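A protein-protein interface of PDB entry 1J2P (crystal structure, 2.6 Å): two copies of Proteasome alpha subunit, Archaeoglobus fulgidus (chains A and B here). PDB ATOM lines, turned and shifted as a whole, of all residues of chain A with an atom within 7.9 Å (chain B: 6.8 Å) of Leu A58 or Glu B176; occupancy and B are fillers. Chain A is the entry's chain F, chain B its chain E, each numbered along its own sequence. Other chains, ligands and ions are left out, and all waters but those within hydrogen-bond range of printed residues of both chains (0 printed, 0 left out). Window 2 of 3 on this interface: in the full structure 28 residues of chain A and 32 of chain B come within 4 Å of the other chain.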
ATOM      1  N   VAL A  54      -1.096 -24.589  25.449  1.00  0.00           N
ATOM      2  CA  VAL A  54      -0.309 -24.617  26.676  1.00  0.00           C
ATOM      3  C   VAL A  54       0.335 -23.259  26.921  1.00  0.00           C
ATOM      4  O   VAL A  54       0.589 -22.501  25.983  1.00  0.00           O
ATOM      5  CB  VAL A  54       0.798 -25.688  26.610  1.00  0.00           C
ATOM      6  CG1 VAL A  54       0.184 -27.072  26.697  1.00  0.00           C
ATOM      7  CG2 VAL A  54       1.587 -25.539  25.316  1.00  0.00           C
ATOM      8  N   GLY A  55       0.598 -22.957  28.187  1.00  0.00           N
ATOM      9  CA  GLY A  55       1.203 -21.684  28.526  1.00  0.00           C
ATOM     10  C   GLY A  55       2.715 -21.668  28.412  1.00  0.00           C
ATOM     11  O   GLY A  55       3.338 -20.618  28.578  1.00  0.00           O
ATOM     12  N   SER A  56       3.311 -22.823  28.128  1.00  0.00           N
ATOM     13  CA  SER A  56       4.761 -22.906  28.006  1.00  0.00           C
ATOM     14  C   SER A  56       5.219 -23.813  26.872  1.00  0.00           C
ATOM     15  O   SER A  56       4.561 -24.796  26.538  1.00  0.00           O
ATOM     16  CB  SER A  56       5.369 -23.396  29.323  1.00  0.00           C
ATOM     17  OG  SER A  56       6.770 -23.569  29.199  1.00  0.00           O
ATOM     18  N   LYS A  57       6.363 -23.472  26.291  1.00  0.00           N
ATOM     19  CA  LYS A  57       6.939 -24.247  25.201  1.00  0.00           C
ATOM     20  C   LYS A  57       7.773 -25.400  25.742  1.00  0.00           C
ATOM     21  O   LYS A  57       8.237 -26.250  24.981  1.00  0.00           O
ATOM     22  CB  LYS A  57       7.824 -23.354  24.331  1.00  0.00           C
ATOM     23  N   LEU A  58       7.977 -25.416  27.055  1.00  0.00           N
ATOM     24  CA  LEU A  58       8.760 -26.466  27.683  1.00  0.00           C
ATOM     25  C   LEU A  58       7.963 -27.755  27.822  1.00  0.00           C
ATOM     26  O   LEU A  58       8.533 -28.825  28.020  1.00  0.00           O
ATOM     27  CB  LEU A  58       9.269 -25.997  29.048  1.00  0.00           C
ATOM     28  CG  LEU A  58      10.554 -25.166  29.011  1.00  0.00           C
ATOM     29  CD1 LEU A  58      10.407 -24.024  28.037  1.00  0.00           C
ATOM     30  CD2 LEU A  58      10.872 -24.653  30.405  1.00  0.00           C
ATOM     31  N   LEU A  59       6.641 -27.652  27.719  1.00  0.00           N
ATOM     32  CA  LEU A  59       5.793 -28.833  27.814  1.00  0.00           C
ATOM     33  C   LEU A  59       5.867 -29.616  26.512  1.00  0.00           C
ATOM     34  O   LEU A  59       5.786 -29.045  25.424  1.00  0.00           O
ATOM     35  CB  LEU A  59       4.337 -28.453  28.082  1.00  0.00           C
ATOM     36  CG  LEU A  59       3.901 -28.109  29.512  1.00  0.00           C
ATOM     37  CD1 LEU A  59       4.623 -26.873  30.004  1.00  0.00           C
ATOM     38  CD2 LEU A  59       2.410 -27.871  29.534  1.00  0.00           C
ATOM     39  N   GLU A  60       6.037 -30.927  26.626  1.00  0.00           N
ATOM     40  CA  GLU A  60       6.112 -31.789  25.459  1.00  0.00           C
ATOM     41  C   GLU A  60       4.691 -31.912  24.931  1.00  0.00           C
ATOM     42  O   GLU A  60       4.065 -32.962  25.027  1.00  0.00           O
ATOM     43  CB  GLU A  60       6.663 -33.157  25.868  1.00  0.00           C
ATOM     44  CG  GLU A  60       6.863 -34.146  24.733  1.00  0.00           C
ATOM     45  CD  GLU A  60       7.678 -33.575  23.595  1.00  0.00           C
ATOM     46  OE1 GLU A  60       7.097 -32.878  22.742  1.00  0.00           O
ATOM     47  OE2 GLU A  60       8.898 -33.809  23.555  1.00  0.00           O
ATOM     48  N   LYS A  61       4.174 -30.821  24.379  1.00  0.00           N
ATOM     49  CA  LYS A  61       2.812 -30.824  23.864  1.00  0.00           C
ATOM     50  C   LYS A  61       2.621 -31.828  22.734  1.00  0.00           C
ATOM     51  O   LYS A  61       1.490 -32.192  22.405  1.00  0.00           O
ATOM     52  N   LEU B 147      10.684 -37.080  29.594  1.00  0.00           N
ATOM     53  CA  LEU B 147      10.857 -36.233  30.775  1.00  0.00           C
ATOM     54  C   LEU B 147       9.483 -35.922  31.376  1.00  0.00           C
ATOM     55  O   LEU B 147       8.637 -35.280  30.742  1.00  0.00           O
ATOM     56  CB  LEU B 147      11.567 -34.925  30.420  1.00  0.00           C
ATOM     57  CG  LEU B 147      11.770 -33.947  31.588  1.00  0.00           C
ATOM     58  CD1 LEU B 147      12.524 -34.627  32.728  1.00  0.00           C
ATOM     59  CD2 LEU B 147      12.534 -32.714  31.103  1.00  0.00           C
ATOM     60  N   GLU B 158       4.258 -33.980  30.696  1.00  0.00           N
ATOM     61  CA  GLU B 158       5.468 -34.305  29.956  1.00  0.00           C
ATOM     62  C   GLU B 158       6.066 -33.004  29.436  1.00  0.00           C
ATOM     63  O   GLU B 158       5.362 -32.175  28.869  1.00  0.00           O
ATOM     64  CB  GLU B 158       5.163 -35.255  28.794  1.00  0.00           C
ATOM     65  CG  GLU B 158       6.404 -35.634  28.010  1.00  0.00           C
ATOM     66  CD  GLU B 158       6.197 -36.816  27.080  1.00  0.00           C
ATOM     67  OE1 GLU B 158       7.107 -37.090  26.261  1.00  0.00           O
ATOM     68  OE2 GLU B 158       5.131 -37.473  27.169  1.00  0.00           O
ATOM     69  N   TYR B 159       7.364 -32.821  29.650  1.00  0.00           N
ATOM     70  CA  TYR B 159       8.053 -31.614  29.210  1.00  0.00           C
ATOM     71  C   TYR B 159       9.226 -31.910  28.280  1.00  0.00           C
ATOM     72  O   TYR B 159       9.619 -33.064  28.089  1.00  0.00           O
ATOM     73  CB  TYR B 159       8.614 -30.844  30.407  1.00  0.00           C
ATOM     74  CG  TYR B 159       7.614 -30.109  31.263  1.00  0.00           C
ATOM     75  CD1 TYR B 159       6.825 -30.783  32.203  1.00  0.00           C
ATOM     76  CD2 TYR B 159       7.498 -28.722  31.178  1.00  0.00           C
ATOM     77  CE1 TYR B 159       5.952 -30.089  33.039  1.00  0.00           C
ATOM     78  CE2 TYR B 159       6.633 -28.017  32.009  1.00  0.00           C
ATOM     79  CZ  TYR B 159       5.865 -28.704  32.936  1.00  0.00           C
ATOM     80  OH  TYR B 159       5.026 -27.990  33.761  1.00  0.00           O
ATOM     81  N   LYS B 160       9.786 -30.843  27.714  1.00  0.00           N
ATOM     82  CA  LYS B 160      10.957 -30.937  26.850  1.00  0.00           C
ATOM     83  C   LYS B 160      12.102 -30.513  27.758  1.00  0.00           C
ATOM     84  O   LYS B 160      13.229 -31.012  27.650  1.00  0.00           O
ATOM     85  CB  LYS B 160      10.873 -29.965  25.674  1.00  0.00           C
ATOM     86  CG  LYS B 160       9.661 -30.112  24.771  1.00  0.00           C
ATOM     87  CD  LYS B 160       9.947 -29.466  23.419  1.00  0.00           C
ATOM     88  CE  LYS B 160       8.706 -29.296  22.568  1.00  0.00           C
ATOM     89  NZ  LYS B 160       7.920 -28.099  22.981  1.00  0.00           N
ATOM     90  N   ALA B 161      11.785 -29.584  28.657  1.00  0.00           N
ATOM     91  CA  ALA B 161      12.734 -29.051  29.632  1.00  0.00           C
ATOM     92  C   ALA B 161      11.915 -28.408  30.749  1.00  0.00           C
ATOM     93  O   ALA B 161      10.873 -27.800  30.481  1.00  0.00           O
ATOM     94  CB  ALA B 161      13.645 -28.011  28.973  1.00  0.00           C
ATOM     95  N   THR B 162      12.369 -28.547  31.993  1.00  0.00           N
ATOM     96  CA  THR B 162      11.650 -27.970  33.122  1.00  0.00           C
ATOM     97  C   THR B 162      12.465 -28.043  34.413  1.00  0.00           C
ATOM     98  O   THR B 162      13.658 -28.344  34.386  1.00  0.00           O
ATOM     99  CB  THR B 162      10.273 -28.681  33.326  1.00  0.00           C
ATOM    100  OG1 THR B 162       9.549 -28.038  34.380  1.00  0.00           O
ATOM    101  CG2 THR B 162      10.461 -30.153  33.673  1.00  0.00           C
ATOM    102  N   ALA B 163      11.820 -27.768  35.542  1.00  0.00           N
ATOM    103  CA  ALA B 163      12.506 -27.806  36.830  1.00  0.00           C
ATOM    104  C   ALA B 163      11.552 -27.813  38.023  1.00  0.00           C
ATOM    105  O   ALA B 163      10.374 -27.481  37.902  1.00  0.00           O
ATOM    106  CB  ALA B 163      13.452 -26.617  36.942  1.00  0.00           C
ATOM    107  N   ALA B 170      13.021 -19.212  37.786  1.00  0.00           N
ATOM    108  CA  ALA B 170      14.183 -18.802  37.025  1.00  0.00           C
ATOM    109  C   ALA B 170      14.434 -19.751  35.859  1.00  0.00           C
ATOM    110  O   ALA B 170      14.322 -19.367  34.697  1.00  0.00           O
ATOM    111  CB  ALA B 170      15.401 -18.752  37.936  1.00  0.00           C
ATOM    112  N   VAL B 171      14.764 -20.998  36.185  1.00  0.00           N
ATOM    113  CA  VAL B 171      15.047 -22.018  35.186  1.00  0.00           C
ATOM    114  C   VAL B 171      13.987 -22.080  34.101  1.00  0.00           C
ATOM    115  O   VAL B 171      14.304 -22.150  32.917  1.00  0.00           O
ATOM    116  CB  VAL B 171      15.162 -23.406  35.839  1.00  0.00           C
ATOM    117  CG1 VAL B 171      15.405 -24.469  34.771  1.00  0.00           C
ATOM    118  CG2 VAL B 171      16.288 -23.407  36.846  1.00  0.00           C
ATOM    119  N   THR B 172      12.726 -22.049  34.510  1.00  0.00           N
ATOM    120  CA  THR B 172      11.614 -22.121  33.570  1.00  0.00           C
ATOM    121  C   THR B 172      11.596 -20.969  32.572  1.00  0.00           C
ATOM    122  O   THR B 172      11.429 -21.187  31.375  1.00  0.00           O
ATOM    123  CB  THR B 172      10.264 -22.153  34.314  1.00  0.00           C
ATOM    124  OG1 THR B 172      10.231 -23.285  35.190  1.00  0.00           O
ATOM    125  CG2 THR B 172       9.111 -22.252  33.324  1.00  0.00           C
ATOM    126  N   GLU B 173      11.753 -19.744  33.067  1.00  0.00           N
ATOM    127  CA  GLU B 173      11.751 -18.573  32.196  1.00  0.00           C
ATOM    128  C   GLU B 173      12.952 -18.606  31.258  1.00  0.00           C
ATOM    129  O   GLU B 173      12.841 -18.253  30.085  1.00  0.00           O
ATOM    130  CB  GLU B 173      11.776 -17.282  33.021  1.00  0.00           C
ATOM    131  CG  GLU B 173      10.507 -17.039  33.823  1.00  0.00           C
ATOM    132  CD  GLU B 173      10.537 -15.729  34.601  1.00  0.00           C
ATOM    133  OE1 GLU B 173       9.579 -15.471  35.372  1.00  0.00           O
ATOM    134  OE2 GLU B 173      11.514 -14.959  34.440  1.00  0.00           O
ATOM    135  N   PHE B 174      14.099 -19.031  31.779  1.00  0.00           N
ATOM    136  CA  PHE B 174      15.297 -19.112  30.962  1.00  0.00           C
ATOM    137  C   PHE B 174      15.060 -20.091  29.817  1.00  0.00           C
ATOM    138  O   PHE B 174      15.238 -19.737  28.654  1.00  0.00           O
ATOM    139  CB  PHE B 174      16.491 -19.569  31.793  1.00  0.00           C
ATOM    140  CG  PHE B 174      17.767 -19.649  31.013  1.00  0.00           C
ATOM    141  CD1 PHE B 174      18.369 -18.494  30.521  1.00  0.00           C
ATOM    142  CD2 PHE B 174      18.356 -20.882  30.738  1.00  0.00           C
ATOM    143  CE1 PHE B 174      19.541 -18.563  29.765  1.00  0.00           C
ATOM    144  CE2 PHE B 174      19.526 -20.963  29.984  1.00  0.00           C
ATOM    145  CZ  PHE B 174      20.119 -19.802  29.496  1.00  0.00           C
ATOM    146  N   PHE B 175      14.658 -21.320  30.140  1.00  0.00           N
ATOM    147  CA  PHE B 175      14.397 -22.314  29.099  1.00  0.00           C
ATOM    148  C   PHE B 175      13.309 -21.816  28.159  1.00  0.00           C
ATOM    149  O   PHE B 175      13.333 -22.084  26.960  1.00  0.00           O
ATOM    150  CB  PHE B 175      13.933 -23.643  29.696  1.00  0.00           C
ATOM    151  CG  PHE B 175      15.025 -24.457  30.313  1.00  0.00           C
ATOM    152  CD1 PHE B 175      16.344 -24.307  29.910  1.00  0.00           C
ATOM    153  CD2 PHE B 175      14.725 -25.412  31.274  1.00  0.00           C
ATOM    154  CE1 PHE B 175      17.346 -25.096  30.454  1.00  0.00           C
ATOM    155  CE2 PHE B 175      15.719 -26.207  31.823  1.00  0.00           C
ATOM    156  CZ  PHE B 175      17.035 -26.047  31.411  1.00  0.00           C
ATOM    157  N   GLU B 176      12.350 -21.097  28.725  1.00  0.00           N
ATOM    158  CA  GLU B 176      11.230 -20.553  27.972  1.00  0.00           C
ATOM    159  C   GLU B 176      11.708 -19.584  26.897  1.00  0.00           C
ATOM    160  O   GLU B 176      11.038 -19.391  25.887  1.00  0.00           O
ATOM    161  CB  GLU B 176      10.269 -19.839  28.932  1.00  0.00           C
ATOM    162  CG  GLU B 176       8.801 -20.240  28.797  1.00  0.00           C
ATOM    163  CD  GLU B 176       7.965 -19.824  30.012  1.00  0.00           C
ATOM    164  OE1 GLU B 176       7.942 -18.616  30.346  1.00  0.00           O
ATOM    165  OE2 GLU B 176       7.331 -20.707  30.635  1.00  0.00           O
ATOM    166  N   LYS B 177      12.875 -18.988  27.107  1.00  0.00           N
ATOM    167  CA  LYS B 177      13.417 -18.032  26.152  1.00  0.00           C
ATOM    168  C   LYS B 177      14.543 -18.571  25.282  1.00  0.00           C
ATOM    169  O   LYS B 177      14.802 -18.025  24.215  1.00  0.00           O
ATOM    170  CB  LYS B 177      13.913 -16.785  26.891  1.00  0.00           C
ATOM    171  CG  LYS B 177      12.811 -15.966  27.552  1.00  0.00           C
ATOM    172  CD  LYS B 177      13.381 -14.860  28.440  1.00  0.00           C
ATOM    173  N   GLU B 178      15.212 -19.636  25.710  1.00  0.00           N
ATOM    174  CA  GLU B 178      16.317 -20.151  24.916  1.00  0.00           C
ATOM    175  C   GLU B 178      16.438 -21.651  24.705  1.00  0.00           C
ATOM    176  O   GLU B 178      17.504 -22.134  24.327  1.00  0.00           O
ATOM    177  CB  GLU B 178      17.634 -19.609  25.473  1.00  0.00           C
ATOM    178  CG  GLU B 178      17.827 -18.129  25.175  1.00  0.00           C
ATOM    179  CD  GLU B 178      19.131 -17.593  25.707  1.00  0.00           C
ATOM    180  OE1 GLU B 178      20.180 -18.205  25.412  1.00  0.00           O
ATOM    181  OE2 GLU B 178      19.104 -16.562  26.415  1.00  0.00           O
ATOM    182  N   TYR B 179      15.362 -22.395  24.937  1.00  0.00           N
ATOM    183  CA  TYR B 179      15.423 -23.834  24.720  1.00  0.00           C
ATOM    184  C   TYR B 179      15.166 -24.110  23.244  1.00  0.00           C
ATOM    185  O   TYR B 179      14.285 -23.503  22.646  1.00  0.00           O
ATOM    186  CB  TYR B 179      14.376 -24.563  25.554  1.00  0.00           C
ATOM    187  CG  TYR B 179      14.300 -26.038  25.240  1.00  0.00           C
ATOM    188  CD1 TYR B 179      15.250 -26.928  25.736  1.00  0.00           C
ATOM    189  CD2 TYR B 179      13.307 -26.537  24.402  1.00  0.00           C
ATOM    190  CE1 TYR B 179      15.210 -28.284  25.404  1.00  0.00           C
ATOM    191  CE2 TYR B 179      13.259 -27.882  24.063  1.00  0.00           C
ATOM    192  CZ  TYR B 179      14.213 -28.751  24.566  1.00  0.00           C
ATOM    193  OH  TYR B 179      14.169 -30.085  24.221  1.00  0.00           O
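Of the printed residues of chain B, Ser A56 touches Glu B176 (3.3 Å). Of the printed residues of chain B, Leu A58 touches Tyr B159 (3.1 Å), Lys B160 (2.4 Å), Ala B161 (2.8 Å), Thr B172 (3.6 Å), Phe B175 (3.3 Å) and Glu B176 (3.6 Å). Of the printed residues of chain B, Leu A59 touches Glu B158, Tyr B159 and Lys B160. Of the printed residues of chain B, Glu A60 touches Glu B158, Tyr B159 and Lys B160. Printed residues of chain A within 4 Å of Lys B160: Lys A57, Leu A58, Leu A59 and Glu A60. Of the printed residues of chain A, Thr B172 touches Leu A58. Glu B178 touches none of the printed residues of chain A. The nearest residue of chain A that does not touch Glu B176 is Gly A55 (4.5 Å).
O of Leu A58 touches CA of Tyr B159, 3.1 Å away. CD2 of Leu A58 touches O of Thr B172, 3.6 Å away. Leu A58 touches Phe B175. CA of Glu B176 touches CD1 of Leu A58, 3.6 Å away. Leu A59 touches Glu B158. Leu A59 touches Tyr B159. Glu A60 touches Tyr B159. N of Lys B160 touches N of Glu A60 (3.9 Å).
OE2 of Glu B176 lies within hydrogen-bond range of OG of Ser A56. NZ of Lys B160 is in hydrogen-bond range of O of Lys A57 (2.7 Å). The backbone carbonyl oxygen (O) of Leu A58 sits close to the backbone NH (N) of Lys B160, at 2.4 Å. The backbone NH (N) of Glu A60 sits at hydrogen-bond distance from the backbone carbonyl oxygen (O) of Glu B158, at 2.7 Å. The backbone NH of Ala B161 sits at hydrogen-bond distance from the backbone carbonyl oxygen of Leu A58, 3.4 Å away. O of Leu A59 is in hydrogen-bond range of NZ of Lys B160 (3.4 Å).
OG of Ser A56 is in hydrogen-bond range of N of Leu A58 (3.1 Å). O of Leu B147 is in hydrogen-bond range of N of Tyr B159.
Of the 17 printed residues of chain B, 7 touch a printed residue of chain A. Printed residues of chain B that touch a printed residue of chain A: Glu B158, Tyr B159, Lys B160, Ala B161, Thr B172, Phe B175 and Glu B176.
No position is printed for both chains. Of the 14 pairs that touch across the chains among the printed residues, none has its exchanged pair printed and touching as well.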
